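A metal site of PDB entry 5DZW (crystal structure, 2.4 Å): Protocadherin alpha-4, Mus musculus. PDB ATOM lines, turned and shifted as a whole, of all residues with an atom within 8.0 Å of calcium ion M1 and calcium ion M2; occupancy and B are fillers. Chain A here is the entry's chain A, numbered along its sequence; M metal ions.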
ATOM      1  N   GLU A   8     -17.275 -12.132 -11.358  1.00  0.00           N
ATOM      2  CA  GLU A   8     -18.099 -12.173 -10.154  1.00  0.00           C
ATOM      3  C   GLU A   8     -17.284 -12.454  -8.894  1.00  0.00           C
ATOM      4  O   GLU A   8     -16.084 -12.741  -8.977  1.00  0.00           O
ATOM      5  CB  GLU A   8     -19.192 -13.226 -10.294  1.00  0.00           C
ATOM      6  CG  GLU A   8     -18.648 -14.620 -10.599  1.00  0.00           C
ATOM      7  CD  GLU A   8     -19.604 -15.713 -10.193  1.00  0.00           C
ATOM      8  OE1 GLU A   8     -20.464 -15.455  -9.324  1.00  0.00           O
ATOM      9  OE2 GLU A   8     -19.492 -16.833 -10.730  1.00  0.00           O
ATOM     10  N   GLU A   9     -17.940 -12.361  -7.740  1.00  0.00           N
ATOM     11  CA  GLU A   9     -17.344 -12.698  -6.446  1.00  0.00           C
ATOM     12  C   GLU A   9     -16.035 -11.943  -6.199  1.00  0.00           C
ATOM     13  O   GLU A   9     -15.117 -12.469  -5.571  1.00  0.00           O
ATOM     14  CB  GLU A   9     -17.097 -14.200  -6.355  1.00  0.00           C
ATOM     15  CG  GLU A   9     -18.314 -15.064  -6.668  1.00  0.00           C
ATOM     16  CD  GLU A   9     -19.318 -15.123  -5.529  1.00  0.00           C
ATOM     17  OE1 GLU A   9     -19.069 -14.502  -4.476  1.00  0.00           O
ATOM     18  OE2 GLU A   9     -20.359 -15.786  -5.692  1.00  0.00           O
ATOM     19  N   ARG A  60     -20.751  -8.016  -2.201  1.00  0.00           N
ATOM     20  CA  ARG A  60     -20.526  -9.286  -2.882  1.00  0.00           C
ATOM     21  C   ARG A  60     -21.428  -9.441  -4.091  1.00  0.00           C
ATOM     22  O   ARG A  60     -22.652  -9.382  -3.976  1.00  0.00           O
ATOM     23  CB  ARG A  60     -20.726 -10.461  -1.924  1.00  0.00           C
ATOM     24  CG  ARG A  60     -20.577 -11.828  -2.581  1.00  0.00           C
ATOM     25  CD  ARG A  60     -20.650 -12.954  -1.555  1.00  0.00           C
ATOM     26  NE  ARG A  60     -20.465 -14.264  -2.158  1.00  0.00           N
ATOM     27  CZ  ARG A  60     -21.459 -15.082  -2.495  1.00  0.00           C
ATOM     28  NH1 ARG A  60     -22.720 -14.728  -2.290  1.00  0.00           N
ATOM     29  NH2 ARG A  60     -21.195 -16.254  -3.047  1.00  0.00           N
ATOM     30  N   ILE A  61     -20.824  -9.647  -5.258  1.00  0.00           N
ATOM     31  CA  ILE A  61     -21.566  -9.826  -6.491  1.00  0.00           C
ATOM     32  C   ILE A  61     -21.623 -11.300  -6.891  1.00  0.00           C
ATOM     33  O   ILE A  61     -20.708 -11.811  -7.536  1.00  0.00           O
ATOM     34  CB  ILE A  61     -20.952  -9.001  -7.644  1.00  0.00           C
ATOM     35  CG1 ILE A  61     -20.768  -7.545  -7.225  1.00  0.00           C
ATOM     36  CG2 ILE A  61     -21.815  -9.101  -8.896  1.00  0.00           C
ATOM     37  CD1 ILE A  61     -20.155  -6.667  -8.291  1.00  0.00           C
ATOM     38  N   ASP A  62     -22.694 -11.969  -6.481  1.00  0.00           N
ATOM     39  CA  ASP A  62     -22.887 -13.383  -6.805  1.00  0.00           C
ATOM     40  C   ASP A  62     -23.679 -13.511  -8.108  1.00  0.00           C
ATOM     41  O   ASP A  62     -24.880 -13.219  -8.144  1.00  0.00           O
ATOM     42  CB  ASP A  62     -23.618 -14.098  -5.665  1.00  0.00           C
ATOM     43  CG  ASP A  62     -23.473 -15.609  -5.724  1.00  0.00           C
ATOM     44  OD1 ASP A  62     -23.317 -16.158  -6.832  1.00  0.00           O
ATOM     45  OD2 ASP A  62     -23.526 -16.246  -4.654  1.00  0.00           O
ATOM     46  N   ARG A  63     -23.002 -13.933  -9.162  1.00  0.00           N
ATOM     47  CA  ARG A  63     -23.584 -13.956 -10.501  1.00  0.00           C
ATOM     48  C   ARG A  63     -24.833 -14.831 -10.593  1.00  0.00           C
ATOM     49  O   ARG A  63     -25.847 -14.410 -11.171  1.00  0.00           O
ATOM     50  CB  ARG A  63     -22.550 -14.435 -11.518  1.00  0.00           C
ATOM     51  CG  ARG A  63     -23.116 -14.595 -12.908  1.00  0.00           C
ATOM     52  CD  ARG A  63     -22.145 -15.323 -13.820  1.00  0.00           C
ATOM     53  NE  ARG A  63     -22.828 -15.867 -14.983  1.00  0.00           N
ATOM     54  CZ  ARG A  63     -23.477 -17.026 -14.991  1.00  0.00           C
ATOM     55  NH1 ARG A  63     -24.077 -17.450 -16.090  1.00  0.00           N
ATOM     56  NH2 ARG A  63     -23.529 -17.768 -13.885  1.00  0.00           N
ATOM     57  N   GLU A  64     -24.760 -16.029 -10.035  1.00  0.00           N
ATOM     58  CA  GLU A  64     -25.853 -16.996 -10.127  1.00  0.00           C
ATOM     59  C   GLU A  64     -27.097 -16.531  -9.380  1.00  0.00           C
ATOM     60  O   GLU A  64     -28.196 -17.023  -9.625  1.00  0.00           O
ATOM     61  CB  GLU A  64     -25.401 -18.357  -9.578  1.00  0.00           C
ATOM     62  CG  GLU A  64     -24.187 -18.957 -10.278  1.00  0.00           C
ATOM     63  CD  GLU A  64     -22.878 -18.472  -9.701  1.00  0.00           C
ATOM     64  OE1 GLU A  64     -22.720 -17.247  -9.508  1.00  0.00           O
ATOM     65  OE2 GLU A  64     -22.002 -19.317  -9.431  1.00  0.00           O
ATOM     66  N   GLU A  65     -26.926 -15.574  -8.465  1.00  0.00           N
ATOM     67  CA  GLU A  65     -28.048 -15.029  -7.721  1.00  0.00           C
ATOM     68  C   GLU A  65     -28.700 -13.898  -8.495  1.00  0.00           C
ATOM     69  O   GLU A  65     -29.803 -13.449  -8.174  1.00  0.00           O
ATOM     70  CB  GLU A  65     -27.591 -14.557  -6.340  1.00  0.00           C
ATOM     71  CG  GLU A  65     -28.729 -14.343  -5.344  1.00  0.00           C
ATOM     72  CD  GLU A  65     -28.227 -14.109  -3.935  1.00  0.00           C
ATOM     73  OE1 GLU A  65     -26.999 -14.164  -3.711  1.00  0.00           O
ATOM     74  OE2 GLU A  65     -29.067 -13.887  -3.027  1.00  0.00           O
ATOM     75  N   GLY A  68     -28.685 -15.961 -12.846  1.00  0.00           N
ATOM     76  CA  GLY A  68     -29.046 -17.354 -12.634  1.00  0.00           C
ATOM     77  C   GLY A  68     -28.470 -18.272 -13.692  1.00  0.00           C
ATOM     78  O   GLY A  68     -27.258 -18.376 -13.841  1.00  0.00           O
ATOM     79  N   ARG A  95     -18.740 -11.582 -15.591  1.00  0.00           N
ATOM     80  CA  ARG A  95     -18.252 -12.844 -16.126  1.00  0.00           C
ATOM     81  C   ARG A  95     -18.342 -13.959 -15.091  1.00  0.00           C
ATOM     82  O   ARG A  95     -18.189 -13.722 -13.895  1.00  0.00           O
ATOM     83  CB  ARG A  95     -16.820 -12.694 -16.643  1.00  0.00           C
ATOM     84  CG  ARG A  95     -16.691 -11.716 -17.790  1.00  0.00           C
ATOM     85  CD  ARG A  95     -15.245 -11.548 -18.247  1.00  0.00           C
ATOM     86  NE  ARG A  95     -14.409 -10.980 -17.204  1.00  0.00           N
ATOM     87  CZ  ARG A  95     -13.172 -10.527 -17.405  1.00  0.00           C
ATOM     88  NH1 ARG A  95     -12.641 -10.556 -18.620  1.00  0.00           N
ATOM     89  NH2 ARG A  95     -12.479 -10.023 -16.396  1.00  0.00           N
ATOM     90  N   ASP A  96     -18.581 -15.172 -15.578  1.00  0.00           N
ATOM     91  CA  ASP A  96     -18.774 -16.328 -14.710  1.00  0.00           C
ATOM     92  C   ASP A  96     -17.466 -16.851 -14.132  1.00  0.00           C
ATOM     93  O   ASP A  96     -16.453 -16.924 -14.812  1.00  0.00           O
ATOM     94  CB  ASP A  96     -19.488 -17.444 -15.474  1.00  0.00           C
ATOM     95  CG  ASP A  96     -19.777 -18.663 -14.621  1.00  0.00           C
ATOM     96  OD1 ASP A  96     -19.562 -19.796 -15.101  1.00  0.00           O
ATOM     97  OD2 ASP A  96     -20.212 -18.489 -13.459  1.00  0.00           O
ATOM     98  N   ILE A  97     -17.507 -17.207 -12.847  1.00  0.00           N
ATOM     99  CA  ILE A  97     -16.377 -17.850 -12.181  1.00  0.00           C
ATOM    100  C   ILE A  97     -16.766 -19.239 -11.705  1.00  0.00           C
ATOM    101  O   ILE A  97     -17.802 -19.412 -11.051  1.00  0.00           O
ATOM    102  CB  ILE A  97     -15.876 -17.010 -10.992  1.00  0.00           C
ATOM    103  CG1 ILE A  97     -15.144 -15.765 -11.482  1.00  0.00           C
ATOM    104  CG2 ILE A  97     -14.959 -17.832 -10.091  1.00  0.00           C
ATOM    105  CD1 ILE A  97     -14.397 -15.020 -10.396  1.00  0.00           C
ATOM    106  N   ASN A  98     -15.945 -20.232 -12.031  1.00  0.00           N
ATOM    107  CA  ASN A  98     -16.219 -21.612 -11.638  1.00  0.00           C
ATOM    108  C   ASN A  98     -16.048 -21.819 -10.137  1.00  0.00           C
ATOM    109  O   ASN A  98     -15.084 -22.429  -9.692  1.00  0.00           O
ATOM    110  CB  ASN A  98     -15.306 -22.582 -12.400  1.00  0.00           C
ATOM    111  CG  ASN A  98     -15.772 -24.022 -12.319  1.00  0.00           C
ATOM    112  OD1 ASN A  98     -16.913 -24.292 -11.942  1.00  0.00           O
ATOM    113  ND2 ASN A  98     -14.894 -24.949 -12.677  1.00  0.00           N
ATOM    114  N   ASP A  99     -16.989 -21.290  -9.360  1.00  0.00           N
ATOM    115  CA  ASP A  99     -16.905 -21.372  -7.903  1.00  0.00           C
ATOM    116  C   ASP A  99     -17.961 -22.300  -7.316  1.00  0.00           C
ATOM    117  O   ASP A  99     -18.162 -22.353  -6.103  1.00  0.00           O
ATOM    118  CB  ASP A  99     -17.020 -19.978  -7.271  1.00  0.00           C
ATOM    119  CG  ASP A  99     -18.361 -19.314  -7.552  1.00  0.00           C
ATOM    120  OD1 ASP A  99     -18.999 -19.647  -8.569  1.00  0.00           O
ATOM    121  OD2 ASP A  99     -18.774 -18.450  -6.740  1.00  0.00           O
ATOM    122  N   ASN A 100     -18.651 -23.038  -8.190  1.00  0.00           N
ATOM    123  CA  ASN A 100     -19.617 -24.047  -7.753  1.00  0.00           C
ATOM    124  C   ASN A 100     -19.345 -25.411  -8.380  1.00  0.00           C
ATOM    125  O   ASN A 100     -19.205 -25.520  -9.594  1.00  0.00           O
ATOM    126  CB  ASN A 100     -21.037 -23.591  -8.078  1.00  0.00           C
ATOM    127  CG  ASN A 100     -21.532 -22.501  -7.162  1.00  0.00           C
ATOM    128  OD1 ASN A 100     -21.029 -22.327  -6.053  1.00  0.00           O
ATOM    129  ND2 ASN A 100     -22.527 -21.750  -7.618  1.00  0.00           N
ATOM    130  N   ASP A 130     -25.487 -28.177 -12.242  1.00  0.00           N
ATOM    131  CA  ASP A 130     -24.481 -27.163 -11.950  1.00  0.00           C
ATOM    132  C   ASP A 130     -25.087 -25.768 -12.019  1.00  0.00           C
ATOM    133  O   ASP A 130     -25.864 -25.462 -12.928  1.00  0.00           O
ATOM    134  CB  ASP A 130     -23.298 -27.282 -12.904  1.00  0.00           C
ATOM    135  CG  ASP A 130     -22.064 -26.565 -12.406  1.00  0.00           C
ATOM    136  OD1 ASP A 130     -21.784 -26.648 -11.187  1.00  0.00           O
ATOM    137  OD2 ASP A 130     -21.389 -25.907 -13.221  1.00  0.00           O
ATOM    138  N   ALA A 131     -24.743 -24.927 -11.053  1.00  0.00           N
ATOM    139  CA  ALA A 131     -25.279 -23.575 -10.983  1.00  0.00           C
ATOM    140  C   ALA A 131     -24.626 -22.652 -12.007  1.00  0.00           C
ATOM    141  O   ALA A 131     -25.235 -21.705 -12.489  1.00  0.00           O
ATOM    142  CB  ALA A 131     -25.115 -23.008  -9.577  1.00  0.00           C
ATOM    143  N   ASP A 132     -23.364 -22.951 -12.338  1.00  0.00           N
ATOM    144  CA  ASP A 132     -22.607 -22.138 -13.271  1.00  0.00           C
ATOM    145  C   ASP A 132     -23.087 -22.345 -14.707  1.00  0.00           C
ATOM    146  O   ASP A 132     -23.836 -23.277 -14.990  1.00  0.00           O
ATOM    147  CB  ASP A 132     -21.117 -22.461 -13.160  1.00  0.00           C
ATOM    148  CG  ASP A 132     -20.568 -22.200 -11.773  1.00  0.00           C
ATOM    149  OD1 ASP A 132     -21.384 -22.005 -10.840  1.00  0.00           O
ATOM    150  OD2 ASP A 132     -19.334 -22.203 -11.606  1.00  0.00           O
ATOM    151  N   ILE A 133     -22.653 -21.465 -15.604  1.00  0.00           N
ATOM    152  CA  ILE A 133     -23.053 -21.526 -17.002  1.00  0.00           C
ATOM    153  C   ILE A 133     -21.850 -21.368 -17.922  1.00  0.00           C
ATOM    154  O   ILE A 133     -21.022 -20.477 -17.717  1.00  0.00           O
ATOM    155  CB  ILE A 133     -24.106 -20.449 -17.347  1.00  0.00           C
ATOM    156  CG1 ILE A 133     -25.389 -20.648 -16.515  1.00  0.00           C
ATOM    157  CG2 ILE A 133     -24.449 -20.481 -18.831  1.00  0.00           C
ATOM    158  CD1 ILE A 133     -26.122 -21.937 -16.821  1.00  0.00           C
ATOM    159  N   ASN A 136     -17.689 -23.767 -17.499  1.00  0.00           N
ATOM    160  CA  ASN A 136     -17.734 -24.126 -16.082  1.00  0.00           C
ATOM    161  C   ASN A 136     -18.880 -25.081 -15.778  1.00  0.00           C
ATOM    162  O   ASN A 136     -18.928 -25.676 -14.705  1.00  0.00           O
ATOM    163  CB  ASN A 136     -17.850 -22.872 -15.219  1.00  0.00           C
ATOM    164  CG  ASN A 136     -16.749 -21.863 -15.490  1.00  0.00           C
ATOM    165  OD1 ASN A 136     -15.670 -22.220 -15.961  1.00  0.00           O
ATOM    166  ND2 ASN A 136     -17.018 -20.593 -15.195  1.00  0.00           N
HETATM  167 CA    CA M   1     -20.758 -17.680  -8.068  1.00  0.00          CA
HETATM  168 CA    CA M   2     -20.333 -19.026 -11.171  1.00  0.00          CA
HETATM  169 CA    CA M   3     -19.276 -25.117 -12.067  1.00  0.00          CA
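NH2 of Arg 63 lies close to OD2 of Asp 96.
The side-chain amide nitrogen of Asn 136 sits at hydrogen-bond distance from the side-chain carboxylate of Asp 96 (2.7 Å).
The side-chain carboxylate of Glu 64 sits close to the side-chain amide nitrogen of Asn 100.
N of Asp 99 sits at hydrogen-bond distance from OD2 of Asp 132 (3.4 Å).
The side-chain carboxylate (OE1) of Glu 9 is in salt-bridge range of the guanidinium group (NE) of Arg 60, at 2.7 Å.
The backbone NH (N) of Glu 9 sits at hydrogen-bond distance from the backbone carbonyl oxygen (O) of Ile 61 (2.8 Å).
ND2 of Asn 100 lies close to OD1 of Asp 132, at 3.4 Å.
The guanidinium group (NH2) of Arg 60 lies within salt-bridge range of the side-chain carboxylate (OD2) of Asp 62, 2.8 Å away.
Residues that only touch calcium ion M1: Asp 62 (3.2 Å).
Of the 20 residues printed, 5 come within 4 Å of calcium ion M1.
The nearest printed residue that does not touch calcium ion M1 is Asn 100 (4.5 Å).
Residues that only touch calcium ion M2: Asp 132 (3.2 Å).
Six residues have an atom within 4 Å of calcium ion M2: Glu 8, Glu 64, Asp 96, Ile 97, Asp 99 and Asp 132.
The nearest printed residue that does not touch calcium ion M2 is Arg 63 (4.4 Å).
OE2 of Glu 64 binds calcium ion M1, 2.5 Å away.
Calcium ion M1 is bound by OE1 of Glu 64, 2.5 Å away.
Calcium ion M1 is bound by the side-chain carboxylate (OD2) of Asp 99, 2.5 Å away.
Calcium ion M1 is bound by OE1 of Glu 8, at 2.6 Å.
OD1 of Asp 99 binds calcium ion M1.
Calcium ion M1 has five donor atoms within binding distance.
Slightly farther from calcium ion M1 lies OE2 of Glu 9 (3.1 Å).
Slightly farther from calcium ion M1 lies OE2 of Glu 8 (3.1 Å).
Calcium ion M2 is bound by the side-chain carboxylate of Asp 96 (2.4 Å), the side-chain carboxylate of Glu 8 (2.4 Å), the side-chain carboxylate of Glu 64 (2.4 Å) and the backbone carbonyl oxygen of Ile 97 (2.6 Å).
Calcium ion M2 has four donor atoms within binding distance.
Slightly farther from calcium ion M2 lies the side-chain carboxylate (OD1) of Asp 99 (3.0 Å).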
